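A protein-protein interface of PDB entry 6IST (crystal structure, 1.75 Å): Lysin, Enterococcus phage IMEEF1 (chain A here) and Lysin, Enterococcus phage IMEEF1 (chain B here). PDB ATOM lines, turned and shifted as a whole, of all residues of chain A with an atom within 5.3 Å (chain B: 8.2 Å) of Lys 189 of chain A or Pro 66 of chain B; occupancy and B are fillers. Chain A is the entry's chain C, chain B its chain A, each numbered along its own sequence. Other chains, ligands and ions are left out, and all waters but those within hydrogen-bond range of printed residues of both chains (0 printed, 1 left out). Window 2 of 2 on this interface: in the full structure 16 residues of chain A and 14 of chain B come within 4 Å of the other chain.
Of the 11 printed residues of chain A, 6 touch a printed residue of chain B. Hydrophobic or aromatic side chains of chain A within 4 Å of the printed part of chain B: Phe 184, Ile 186, Ile 191 and Val 235. Among the printed residues, 7 pairs touch across the chains.
The guanidinium group of Arg 23 of chain B lies within hydrogen-bond range of the backbone carbonyl oxygen of Leu 65 of chain B, 2.7 Å away. N of Arg 23 of chain B sits at hydrogen-bond distance from O of Pro 66 of chain B. The backbone carbonyl oxygen (O) of Phe 184 of chain A is in hydrogen-bond range of the backbone NH (N) of Ile 191 of chain A (2.7 Å). N of Val 235 of chain A lies within hydrogen-bond range of O of Arg 190 of chain A (3.0 Å).
Among the printed residues, pairs that only touch across the chains: Phe 184 of chain A with Met 60 of chain B, Ile 186 of chain A with Ala 64 of chain B, Gly 187 of chain A with Leu 65 of chain B, Lys 189 of chain A with Pro 66 of chain B, Ile 191 of chain A with Met 60 of chain B and Val 235 of chain A with Ala 63 of chain B.
Of the printed residues of chain B, Phe 184 of chain A touches Met 60 (3.96 Å). Printed residues of chain B within 4 Å of Gly 187 of chain A: Leu 65. No residue of chain B comes within 4 Å of Gly 188 of chain A. Of the printed residues of chain B, Ile 191 of chain A touches Met 60. Printed residues of chain A within 4 Å of Ala 63 of chain B: Val 235 (3.8 Å). Of chain A, only Lys 189 comes within 4 Å of Pro 66 of chain B. The nearest residue of chain B that does not touch Lys 189 of chain A is Leu 65 of chain B (4.9 Å). The nearest printed residue of chain B that does not touch Phe 184 of chain A is Met 61 of chain B (6.2 Å).
O of Ala 64 of chain B lies within hydrogen-bond range of NZ of Lys 189 of chain A (2.8 Å).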
ATOM      1  N   PHE A 184      -6.401 -12.400 -19.381  1.00  0.00           N
ATOM      2  CA  PHE A 184      -7.820 -11.982 -19.470  1.00  0.00           C
ATOM      3  C   PHE A 184      -8.026 -10.733 -18.691  1.00  0.00           C
ATOM      4  O   PHE A 184      -7.706 -10.678 -17.532  1.00  0.00           O
ATOM      5  CB  PHE A 184      -8.650 -13.116 -18.976  1.00  0.00           C
ATOM      6  CG  PHE A 184     -10.146 -12.922 -19.019  1.00  0.00           C
ATOM      7  CD1 PHE A 184     -10.777 -12.403 -20.106  1.00  0.00           C
ATOM      8  CD2 PHE A 184     -10.904 -13.362 -17.948  1.00  0.00           C
ATOM      9  CE1 PHE A 184     -12.146 -12.266 -20.114  1.00  0.00           C
ATOM     10  CE2 PHE A 184     -12.283 -13.260 -17.945  1.00  0.00           C
ATOM     11  CZ  PHE A 184     -12.898 -12.691 -19.044  1.00  0.00           C
ATOM     12  N   VAL A 185      -8.610  -9.731 -19.335  1.00  0.00           N
ATOM     13  CA  VAL A 185      -8.963  -8.495 -18.693  1.00  0.00           C
ATOM     14  C   VAL A 185     -10.435  -8.524 -18.397  1.00  0.00           C
ATOM     15  O   VAL A 185     -11.238  -8.807 -19.290  1.00  0.00           O
ATOM     16  CB  VAL A 185      -8.608  -7.309 -19.627  1.00  0.00           C
ATOM     17  CG1 VAL A 185      -9.094  -5.980 -19.070  1.00  0.00           C
ATOM     18  CG2 VAL A 185      -7.111  -7.331 -19.857  1.00  0.00           C
ATOM     19  N   ILE A 186     -10.769  -8.299 -17.126  1.00  0.00           N
ATOM     20  CA  ILE A 186     -12.139  -8.295 -16.663  1.00  0.00           C
ATOM     21  C   ILE A 186     -12.216  -7.494 -15.369  1.00  0.00           C
ATOM     22  O   ILE A 186     -11.350  -7.625 -14.521  1.00  0.00           O
ATOM     23  CB  ILE A 186     -12.652  -9.741 -16.408  1.00  0.00           C
ATOM     24  CG1 ILE A 186     -14.081  -9.735 -15.865  1.00  0.00           C
ATOM     25  CG2 ILE A 186     -11.725 -10.516 -15.495  1.00  0.00           C
ATOM     26  CD1 ILE A 186     -14.819 -11.041 -15.927  1.00  0.00           C
ATOM     27  N   GLY A 187     -13.264  -6.692 -15.255  1.00  0.00           N
ATOM     28  CA  GLY A 187     -13.480  -5.829 -14.052  1.00  0.00           C
ATOM     29  C   GLY A 187     -12.323  -4.909 -13.710  1.00  0.00           C
ATOM     30  O   GLY A 187     -12.064  -4.655 -12.549  1.00  0.00           O
ATOM     31  N   GLY A 188     -11.616  -4.407 -14.712  1.00  0.00           N
ATOM     32  CA  GLY A 188     -10.470  -3.567 -14.446  1.00  0.00           C
ATOM     33  C   GLY A 188      -9.280  -4.328 -13.879  1.00  0.00           C
ATOM     34  O   GLY A 188      -8.381  -3.702 -13.347  1.00  0.00           O
ATOM     35  N   LYS A 189      -9.273  -5.651 -14.004  1.00  0.00           N
ATOM     36  CA  LYS A 189      -8.171  -6.487 -13.517  1.00  0.00           C
ATOM     37  C   LYS A 189      -7.635  -7.364 -14.663  1.00  0.00           C
ATOM     38  O   LYS A 189      -8.224  -7.497 -15.704  1.00  0.00           O
ATOM     39  CB  LYS A 189      -8.591  -7.431 -12.394  1.00  0.00           C
ATOM     40  CG  LYS A 189      -9.453  -6.877 -11.278  1.00  0.00           C
ATOM     41  CD  LYS A 189      -8.814  -5.711 -10.613  1.00  0.00           C
ATOM     42  CE  LYS A 189      -9.341  -5.472  -9.200  1.00  0.00           C
ATOM     43  NZ  LYS A 189     -10.793  -5.653  -9.022  1.00  0.00           N
ATOM     44  N   ARG A 190      -6.506  -7.967 -14.434  1.00  0.00           N
ATOM     45  CA  ARG A 190      -5.964  -8.878 -15.400  1.00  0.00           C
ATOM     46  C   ARG A 190      -5.684 -10.241 -14.766  1.00  0.00           C
ATOM     47  O   ARG A 190      -5.175 -10.351 -13.656  1.00  0.00           O
ATOM     48  CB  ARG A 190      -4.782  -8.283 -16.122  1.00  0.00           C
ATOM     49  CG  ARG A 190      -3.577  -8.051 -15.309  1.00  0.00           C
ATOM     50  CD  ARG A 190      -2.614  -7.098 -16.056  1.00  0.00           C
ATOM     51  NE  ARG A 190      -1.657  -6.627 -15.069  1.00  0.00           N
ATOM     52  CZ  ARG A 190      -0.546  -7.249 -14.717  1.00  0.00           C
ATOM     53  NH1 ARG A 190      -0.127  -8.354 -15.327  1.00  0.00           N
ATOM     54  NH2 ARG A 190       0.194  -6.720 -13.766  1.00  0.00           N
ATOM     55  N   ILE A 191      -6.038 -11.289 -15.463  1.00  0.00           N
ATOM     56  CA  ILE A 191      -5.884 -12.658 -14.947  1.00  0.00           C
ATOM     57  C   ILE A 191      -5.043 -13.462 -15.903  1.00  0.00           C
ATOM     58  O   ILE A 191      -5.369 -13.521 -17.046  1.00  0.00           O
ATOM     59  CB  ILE A 191      -7.246 -13.347 -14.807  1.00  0.00           C
ATOM     60  CG1 ILE A 191      -8.148 -12.455 -13.938  1.00  0.00           C
ATOM     61  CG2 ILE A 191      -7.052 -14.771 -14.256  1.00  0.00           C
ATOM     62  CD1 ILE A 191      -9.494 -13.049 -13.563  1.00  0.00           C
ATOM     63  N   LEU A 232      -4.152  -2.131 -14.699  1.00  0.00           N
ATOM     64  CA  LEU A 232      -5.062  -3.232 -14.401  1.00  0.00           C
ATOM     65  C   LEU A 232      -4.332  -4.163 -13.446  1.00  0.00           C
ATOM     66  O   LEU A 232      -3.495  -4.920 -13.866  1.00  0.00           O
ATOM     67  CB  LEU A 232      -5.372  -3.992 -15.668  1.00  0.00           C
ATOM     68  CG  LEU A 232      -5.952  -3.182 -16.838  1.00  0.00           C
ATOM     69  CD1 LEU A 232      -5.881  -4.061 -18.079  1.00  0.00           C
ATOM     70  CD2 LEU A 232      -7.378  -2.771 -16.594  1.00  0.00           C
ATOM     71  N   PRO A 233      -4.617  -4.077 -12.152  1.00  0.00           N
ATOM     72  CA  PRO A 233      -3.893  -4.981 -11.260  1.00  0.00           C
ATOM     73  C   PRO A 233      -4.132  -6.444 -11.576  1.00  0.00           C
ATOM     74  O   PRO A 233      -5.209  -6.832 -12.011  1.00  0.00           O
ATOM     75  CB  PRO A 233      -4.477  -4.673  -9.880  1.00  0.00           C
ATOM     76  CG  PRO A 233      -5.230  -3.381 -10.036  1.00  0.00           C
ATOM     77  CD  PRO A 233      -5.646  -3.314 -11.475  1.00  0.00           C
ATOM     78  N   VAL A 235      -4.924 -10.221 -10.684  1.00  0.00           N
ATOM     79  CA  VAL A 235      -5.514 -11.077  -9.683  1.00  0.00           C
ATOM     80  C   VAL A 235      -5.365 -12.524 -10.101  1.00  0.00           C
ATOM     81  O   VAL A 235      -5.328 -12.826 -11.282  1.00  0.00           O
ATOM     82  CB  VAL A 235      -6.994 -10.739  -9.422  1.00  0.00           C
ATOM     83  CG1 VAL A 235      -7.146  -9.309  -8.901  1.00  0.00           C
ATOM     84  CG2 VAL A 235      -7.836 -10.975 -10.657  1.00  0.00           C
ATOM     85  N   TRP B  16     -26.724 -13.106  -8.120  1.00  0.00           N
ATOM     86  CA  TRP B  16     -25.701 -12.102  -7.918  1.00  0.00           C
ATOM     87  C   TRP B  16     -25.771 -11.009  -8.969  1.00  0.00           C
ATOM     88  O   TRP B  16     -26.041 -11.284 -10.090  1.00  0.00           O
ATOM     89  CB  TRP B  16     -24.346 -12.778  -8.007  1.00  0.00           C
ATOM     90  CG  TRP B  16     -24.034 -13.679  -6.875  1.00  0.00           C
ATOM     91  CD1 TRP B  16     -24.495 -14.933  -6.660  1.00  0.00           C
ATOM     92  CD2 TRP B  16     -23.206 -13.353  -5.758  1.00  0.00           C
ATOM     93  NE1 TRP B  16     -23.984 -15.443  -5.477  1.00  0.00           N
ATOM     94  CE2 TRP B  16     -23.220 -14.481  -4.883  1.00  0.00           C
ATOM     95  CE3 TRP B  16     -22.498 -12.210  -5.392  1.00  0.00           C
ATOM     96  CZ2 TRP B  16     -22.485 -14.512  -3.698  1.00  0.00           C
ATOM     97  CZ3 TRP B  16     -21.797 -12.214  -4.225  1.00  0.00           C
ATOM     98  CH2 TRP B  16     -21.764 -13.366  -3.387  1.00  0.00           C
ATOM     99  N   PHE B  17     -25.425  -9.796  -8.575  1.00  0.00           N
ATOM    100  CA  PHE B  17     -25.562  -8.600  -9.408  1.00  0.00           C
ATOM    101  C   PHE B  17     -24.181  -8.016  -9.565  1.00  0.00           C
ATOM    102  O   PHE B  17     -23.546  -7.758  -8.596  1.00  0.00           O
ATOM    103  CB  PHE B  17     -26.498  -7.589  -8.748  1.00  0.00           C
ATOM    104  CG  PHE B  17     -26.755  -6.345  -9.546  1.00  0.00           C
ATOM    105  CD1 PHE B  17     -26.835  -6.366 -10.931  1.00  0.00           C
ATOM    106  CD2 PHE B  17     -26.860  -5.119  -8.896  1.00  0.00           C
ATOM    107  CE1 PHE B  17     -27.088  -5.219 -11.628  1.00  0.00           C
ATOM    108  CE2 PHE B  17     -27.132  -3.950  -9.607  1.00  0.00           C
ATOM    109  CZ  PHE B  17     -27.197  -4.002 -10.976  1.00  0.00           C
ATOM    110  N   VAL B  18     -23.733  -7.891 -10.812  1.00  0.00           N
ATOM    111  CA  VAL B  18     -22.429  -7.266 -11.127  1.00  0.00           C
ATOM    112  C   VAL B  18     -22.650  -5.841 -11.500  1.00  0.00           C
ATOM    113  O   VAL B  18     -23.454  -5.540 -12.372  1.00  0.00           O
ATOM    114  CB  VAL B  18     -21.715  -8.050 -12.255  1.00  0.00           C
ATOM    115  CG1 VAL B  18     -20.434  -7.297 -12.671  1.00  0.00           C
ATOM    116  CG2 VAL B  18     -21.332  -9.416 -11.748  1.00  0.00           C
ATOM    117  N   ILE B  19     -22.004  -4.927 -10.776  1.00  0.00           N
ATOM    118  CA  ILE B  19     -22.163  -3.509 -11.009  1.00  0.00           C
ATOM    119  C   ILE B  19     -20.922  -2.805 -10.530  1.00  0.00           C
ATOM    120  O   ILE B  19     -20.361  -3.192  -9.481  1.00  0.00           O
ATOM    121  CB  ILE B  19     -23.422  -2.949 -10.291  1.00  0.00           C
ATOM    122  CG1 ILE B  19     -23.542  -1.420 -10.506  1.00  0.00           C
ATOM    123  CG2 ILE B  19     -23.400  -3.278  -8.805  1.00  0.00           C
ATOM    124  CD1 ILE B  19     -24.913  -0.819 -10.277  1.00  0.00           C
ATOM    125  N   GLY B  20     -20.457  -1.815 -11.291  1.00  0.00           N
ATOM    126  CA  GLY B  20     -19.316  -1.006 -10.880  1.00  0.00           C
ATOM    127  C   GLY B  20     -18.054  -1.794 -10.553  1.00  0.00           C
ATOM    128  O   GLY B  20     -17.276  -1.404  -9.655  1.00  0.00           O
ATOM    129  N   GLY B  21     -17.841  -2.905 -11.246  1.00  0.00           N
ATOM    130  CA  GLY B  21     -16.731  -3.781 -10.944  1.00  0.00           C
ATOM    131  C   GLY B  21     -16.814  -4.576  -9.679  1.00  0.00           C
ATOM    132  O   GLY B  21     -15.794  -5.122  -9.239  1.00  0.00           O
ATOM    133  N   LYS B  22     -18.012  -4.669  -9.097  1.00  0.00           N
ATOM    134  CA  LYS B  22     -18.229  -5.334  -7.810  1.00  0.00           C
ATOM    135  C   LYS B  22     -19.351  -6.351  -7.993  1.00  0.00           C
ATOM    136  O   LYS B  22     -20.039  -6.294  -8.990  1.00  0.00           O
ATOM    137  CB  LYS B  22     -18.650  -4.375  -6.691  1.00  0.00           C
ATOM    138  CG  LYS B  22     -17.868  -3.091  -6.608  1.00  0.00           C
ATOM    139  CD  LYS B  22     -16.492  -3.258  -6.052  1.00  0.00           C
ATOM    140  CE  LYS B  22     -15.643  -2.003  -6.263  1.00  0.00           C
ATOM    141  NZ  LYS B  22     -16.201  -0.668  -5.896  1.00  0.00           N
ATOM    142  N   ARG B  23     -19.504  -7.239  -7.026  1.00  0.00           N
ATOM    143  CA  ARG B  23     -20.553  -8.294  -7.028  1.00  0.00           C
ATOM    144  C   ARG B  23     -21.392  -8.082  -5.812  1.00  0.00           C
ATOM    145  O   ARG B  23     -20.842  -7.947  -4.750  1.00  0.00           O
ATOM    146  CB  ARG B  23     -19.956  -9.666  -6.814  1.00  0.00           C
ATOM    147  CG  ARG B  23     -19.340 -10.248  -8.019  1.00  0.00           C
ATOM    148  CD  ARG B  23     -18.729 -11.612  -7.697  1.00  0.00           C
ATOM    149  NE  ARG B  23     -17.647 -11.559  -6.735  1.00  0.00           N
ATOM    150  CZ  ARG B  23     -17.554 -12.241  -5.599  1.00  0.00           C
ATOM    151  NH1 ARG B  23     -18.480 -13.113  -5.186  1.00  0.00           N
ATOM    152  NH2 ARG B  23     -16.483 -12.035  -4.862  1.00  0.00           N
ATOM    153  N   ILE B  24     -22.716  -8.160  -5.960  1.00  0.00           N
ATOM    154  CA  ILE B  24     -23.600  -8.029  -4.838  1.00  0.00           C
ATOM    155  C   ILE B  24     -24.524  -9.243  -4.809  1.00  0.00           C
ATOM    156  O   ILE B  24     -25.197  -9.513  -5.785  1.00  0.00           O
ATOM    157  CB  ILE B  24     -24.467  -6.736  -4.921  1.00  0.00           C
ATOM    158  CG1 ILE B  24     -23.588  -5.459  -4.911  1.00  0.00           C
ATOM    159  CG2 ILE B  24     -25.470  -6.688  -3.737  1.00  0.00           C
ATOM    160  CD1 ILE B  24     -24.391  -4.175  -5.112  1.00  0.00           C
ATOM    161  N   TYR B  25     -24.567  -9.955  -3.700  1.00  0.00           N
ATOM    162  CA  TYR B  25     -25.554 -11.018  -3.500  1.00  0.00           C
ATOM    163  C   TYR B  25     -26.909 -10.415  -3.286  1.00  0.00           C
ATOM    164  O   TYR B  25     -27.059  -9.521  -2.465  1.00  0.00           O
ATOM    165  CB  TYR B  25     -25.154 -11.892  -2.315  1.00  0.00           C
ATOM    166  CG  TYR B  25     -26.234 -12.827  -1.902  1.00  0.00           C
ATOM    167  CD1 TYR B  25     -26.614 -13.884  -2.716  1.00  0.00           C
ATOM    168  CD2 TYR B  25     -26.829 -12.706  -0.655  1.00  0.00           C
ATOM    169  CE1 TYR B  25     -27.630 -14.752  -2.330  1.00  0.00           C
ATOM    170  CE2 TYR B  25     -27.843 -13.570  -0.242  1.00  0.00           C
ATOM    171  CZ  TYR B  25     -28.212 -14.603  -1.057  1.00  0.00           C
ATOM    172  OH  TYR B  25     -29.190 -15.440  -0.629  1.00  0.00           O
ATOM    173  N   MET B  60     -13.102 -16.919 -12.004  1.00  0.00           N
ATOM    174  CA  MET B  60     -12.442 -15.695 -12.475  1.00  0.00           C
ATOM    175  C   MET B  60     -13.278 -14.391 -12.182  1.00  0.00           C
ATOM    176  O   MET B  60     -12.750 -13.404 -11.674  1.00  0.00           O
ATOM    177  CB  MET B  60     -12.097 -15.857 -13.991  1.00  0.00           C
ATOM    178  CG  MET B  60     -10.885 -16.764 -14.274  1.00  0.00           C
ATOM    179  SD  MET B  60     -10.525 -16.810 -16.046  1.00  0.00           S
ATOM    180  CE  MET B  60     -11.964 -17.680 -16.619  1.00  0.00           C
ATOM    181  N   MET B  61     -14.603 -14.429 -12.334  1.00  0.00           N
ATOM    182  CA  MET B  61     -15.429 -13.280 -11.925  1.00  0.00           C
ATOM    183  C   MET B  61     -15.299 -13.039 -10.408  1.00  0.00           C
ATOM    184  O   MET B  61     -15.130 -11.880  -9.986  1.00  0.00           O
ATOM    185  CB  MET B  61     -16.895 -13.482 -12.271  1.00  0.00           C
ATOM    186  CG  MET B  61     -17.211 -13.437 -13.775  1.00  0.00           C
ATOM    187  SD  MET B  61     -19.048 -13.285 -14.195  1.00  0.00           S
ATOM    188  CE  MET B  61     -19.512 -14.955 -13.864  1.00  0.00           C
ATOM    189  N   GLU B  62     -15.274 -14.103  -9.589  1.00  0.00           N
ATOM    190  CA  GLU B  62     -15.267 -13.877  -8.119  1.00  0.00           C
ATOM    191  C   GLU B  62     -13.932 -13.273  -7.677  1.00  0.00           C
ATOM    192  O   GLU B  62     -13.880 -12.433  -6.750  1.00  0.00           O
ATOM    193  CB  GLU B  62     -15.598 -15.159  -7.364  1.00  0.00           C
ATOM    194  CG  GLU B  62     -17.065 -15.595  -7.581  1.00  0.00           C
ATOM    195  CD  GLU B  62     -17.463 -16.886  -6.849  1.00  0.00           C
ATOM    196  OE1 GLU B  62     -16.588 -17.763  -6.639  1.00  0.00           O
ATOM    197  OE2 GLU B  62     -18.659 -17.044  -6.464  1.00  0.00           O
ATOM    198  N   ALA B  63     -12.868 -13.676  -8.352  1.00  0.00           N
ATOM    199  CA  ALA B  63     -11.541 -13.144  -8.080  1.00  0.00           C
ATOM    200  C   ALA B  63     -11.357 -11.705  -8.498  1.00  0.00           C
ATOM    201  O   ALA B  63     -10.539 -10.981  -7.917  1.00  0.00           O
ATOM    202  CB  ALA B  63     -10.500 -14.018  -8.757  1.00  0.00           C
ATOM    203  N   ALA B  64     -11.996 -11.311  -9.591  1.00  0.00           N
ATOM    204  CA  ALA B  64     -11.757 -10.024 -10.161  1.00  0.00           C
ATOM    205  C   ALA B  64     -12.734  -8.945  -9.633  1.00  0.00           C
ATOM    206  O   ALA B  64     -12.444  -7.756  -9.719  1.00  0.00           O
ATOM    207  CB  ALA B  64     -11.848 -10.072 -11.693  1.00  0.00           C
ATOM    208  N   LEU B  65     -13.909  -9.371  -9.143  1.00  0.00           N
ATOM    209  CA  LEU B  65     -14.972  -8.470  -8.796  1.00  0.00           C
ATOM    210  C   LEU B  65     -15.202  -8.662  -7.303  1.00  0.00           C
ATOM    211  O   LEU B  65     -15.888  -9.578  -6.914  1.00  0.00           O
ATOM    212  CB  LEU B  65     -16.237  -8.825  -9.599  1.00  0.00           C
ATOM    213  CG  LEU B  65     -16.116  -8.787 -11.132  1.00  0.00           C
ATOM    214  CD1 LEU B  65     -17.300  -9.498 -11.789  1.00  0.00           C
ATOM    215  CD2 LEU B  65     -15.962  -7.389 -11.662  1.00  0.00           C
ATOM    216  N   PRO B  66     -14.653  -7.761  -6.465  1.00  0.00           N
ATOM    217  CA  PRO B  66     -14.875  -7.882  -5.015  1.00  0.00           C
ATOM    218  C   PRO B  66     -16.340  -7.874  -4.656  1.00  0.00           C
ATOM    219  O   PRO B  66     -17.117  -7.144  -5.260  1.00  0.00           O
ATOM    220  CB  PRO B  66     -14.225  -6.609  -4.451  1.00  0.00           C
ATOM    221  CG  PRO B  66     -13.256  -6.178  -5.506  1.00  0.00           C
ATOM    222  CD  PRO B  66     -13.845  -6.578  -6.810  1.00  0.00           C
ATOM    223  N   GLN B  67     -16.702  -8.608  -3.617  1.00  0.00           N
ATOM    224  CA  GLN B  67     -18.093  -8.567  -3.093  1.00  0.00           C
ATOM    225  C   GLN B  67     -18.327  -7.303  -2.260  1.00  0.00           C
ATOM    226  O   GLN B  67     -17.512  -6.971  -1.443  1.00  0.00           O
ATOM    227  CB  GLN B  67     -18.385  -9.766  -2.176  1.00  0.00           C
ATOM    228  CG  GLN B  67     -19.822  -9.839  -1.696  1.00  0.00           C
ATOM    229  CD  GLN B  67     -20.203 -11.131  -0.921  1.00  0.00           C
ATOM    230  OE1 GLN B  67     -21.378 -11.310  -0.548  1.00  0.00           O
ATOM    231  NE2 GLN B  67     -19.232 -12.002  -0.682  1.00  0.00           N
ATOM    232  N   VAL B  68     -19.464  -6.655  -2.413  1.00  0.00           N
ATOM    233  CA  VAL B  68     -19.894  -5.600  -1.450  1.00  0.00           C
ATOM    234  C   VAL B  68     -21.262  -5.980  -0.952  1.00  0.00           C
ATOM    235  O   VAL B  68     -22.018  -6.637  -1.647  1.00  0.00           O
ATOM    236  CB  VAL B  68     -19.934  -4.189  -2.025  1.00  0.00           C
ATOM    237  CG1 VAL B  68     -18.546  -3.723  -2.464  1.00  0.00           C
ATOM    238  CG2 VAL B  68     -20.903  -4.071  -3.165  1.00  0.00           C
ATOM    239  N   LYS B  69     -21.548  -5.610   0.282  1.00  0.00           N
ATOM    240  CA  LYS B  69     -22.776  -6.006   0.971  1.00  0.00           C
ATOM    241  C   LYS B  69     -23.712  -4.860   0.865  1.00  0.00           C
ATOM    242  O   LYS B  69     -23.287  -3.722   1.014  1.00  0.00           O
ATOM    243  CB  LYS B  69     -22.492  -6.233   2.453  1.00  0.00           C
ATOM    244  CG  LYS B  69     -21.445  -7.290   2.725  1.00  0.00           C
ATOM    245  CD  LYS B  69     -21.997  -8.670   2.485  1.00  0.00           C
ATOM    246  CE  LYS B  69     -20.933  -9.708   2.797  1.00  0.00           C
ATOM    247  NZ  LYS B  69     -21.337 -11.040   2.253  1.00  0.00           N
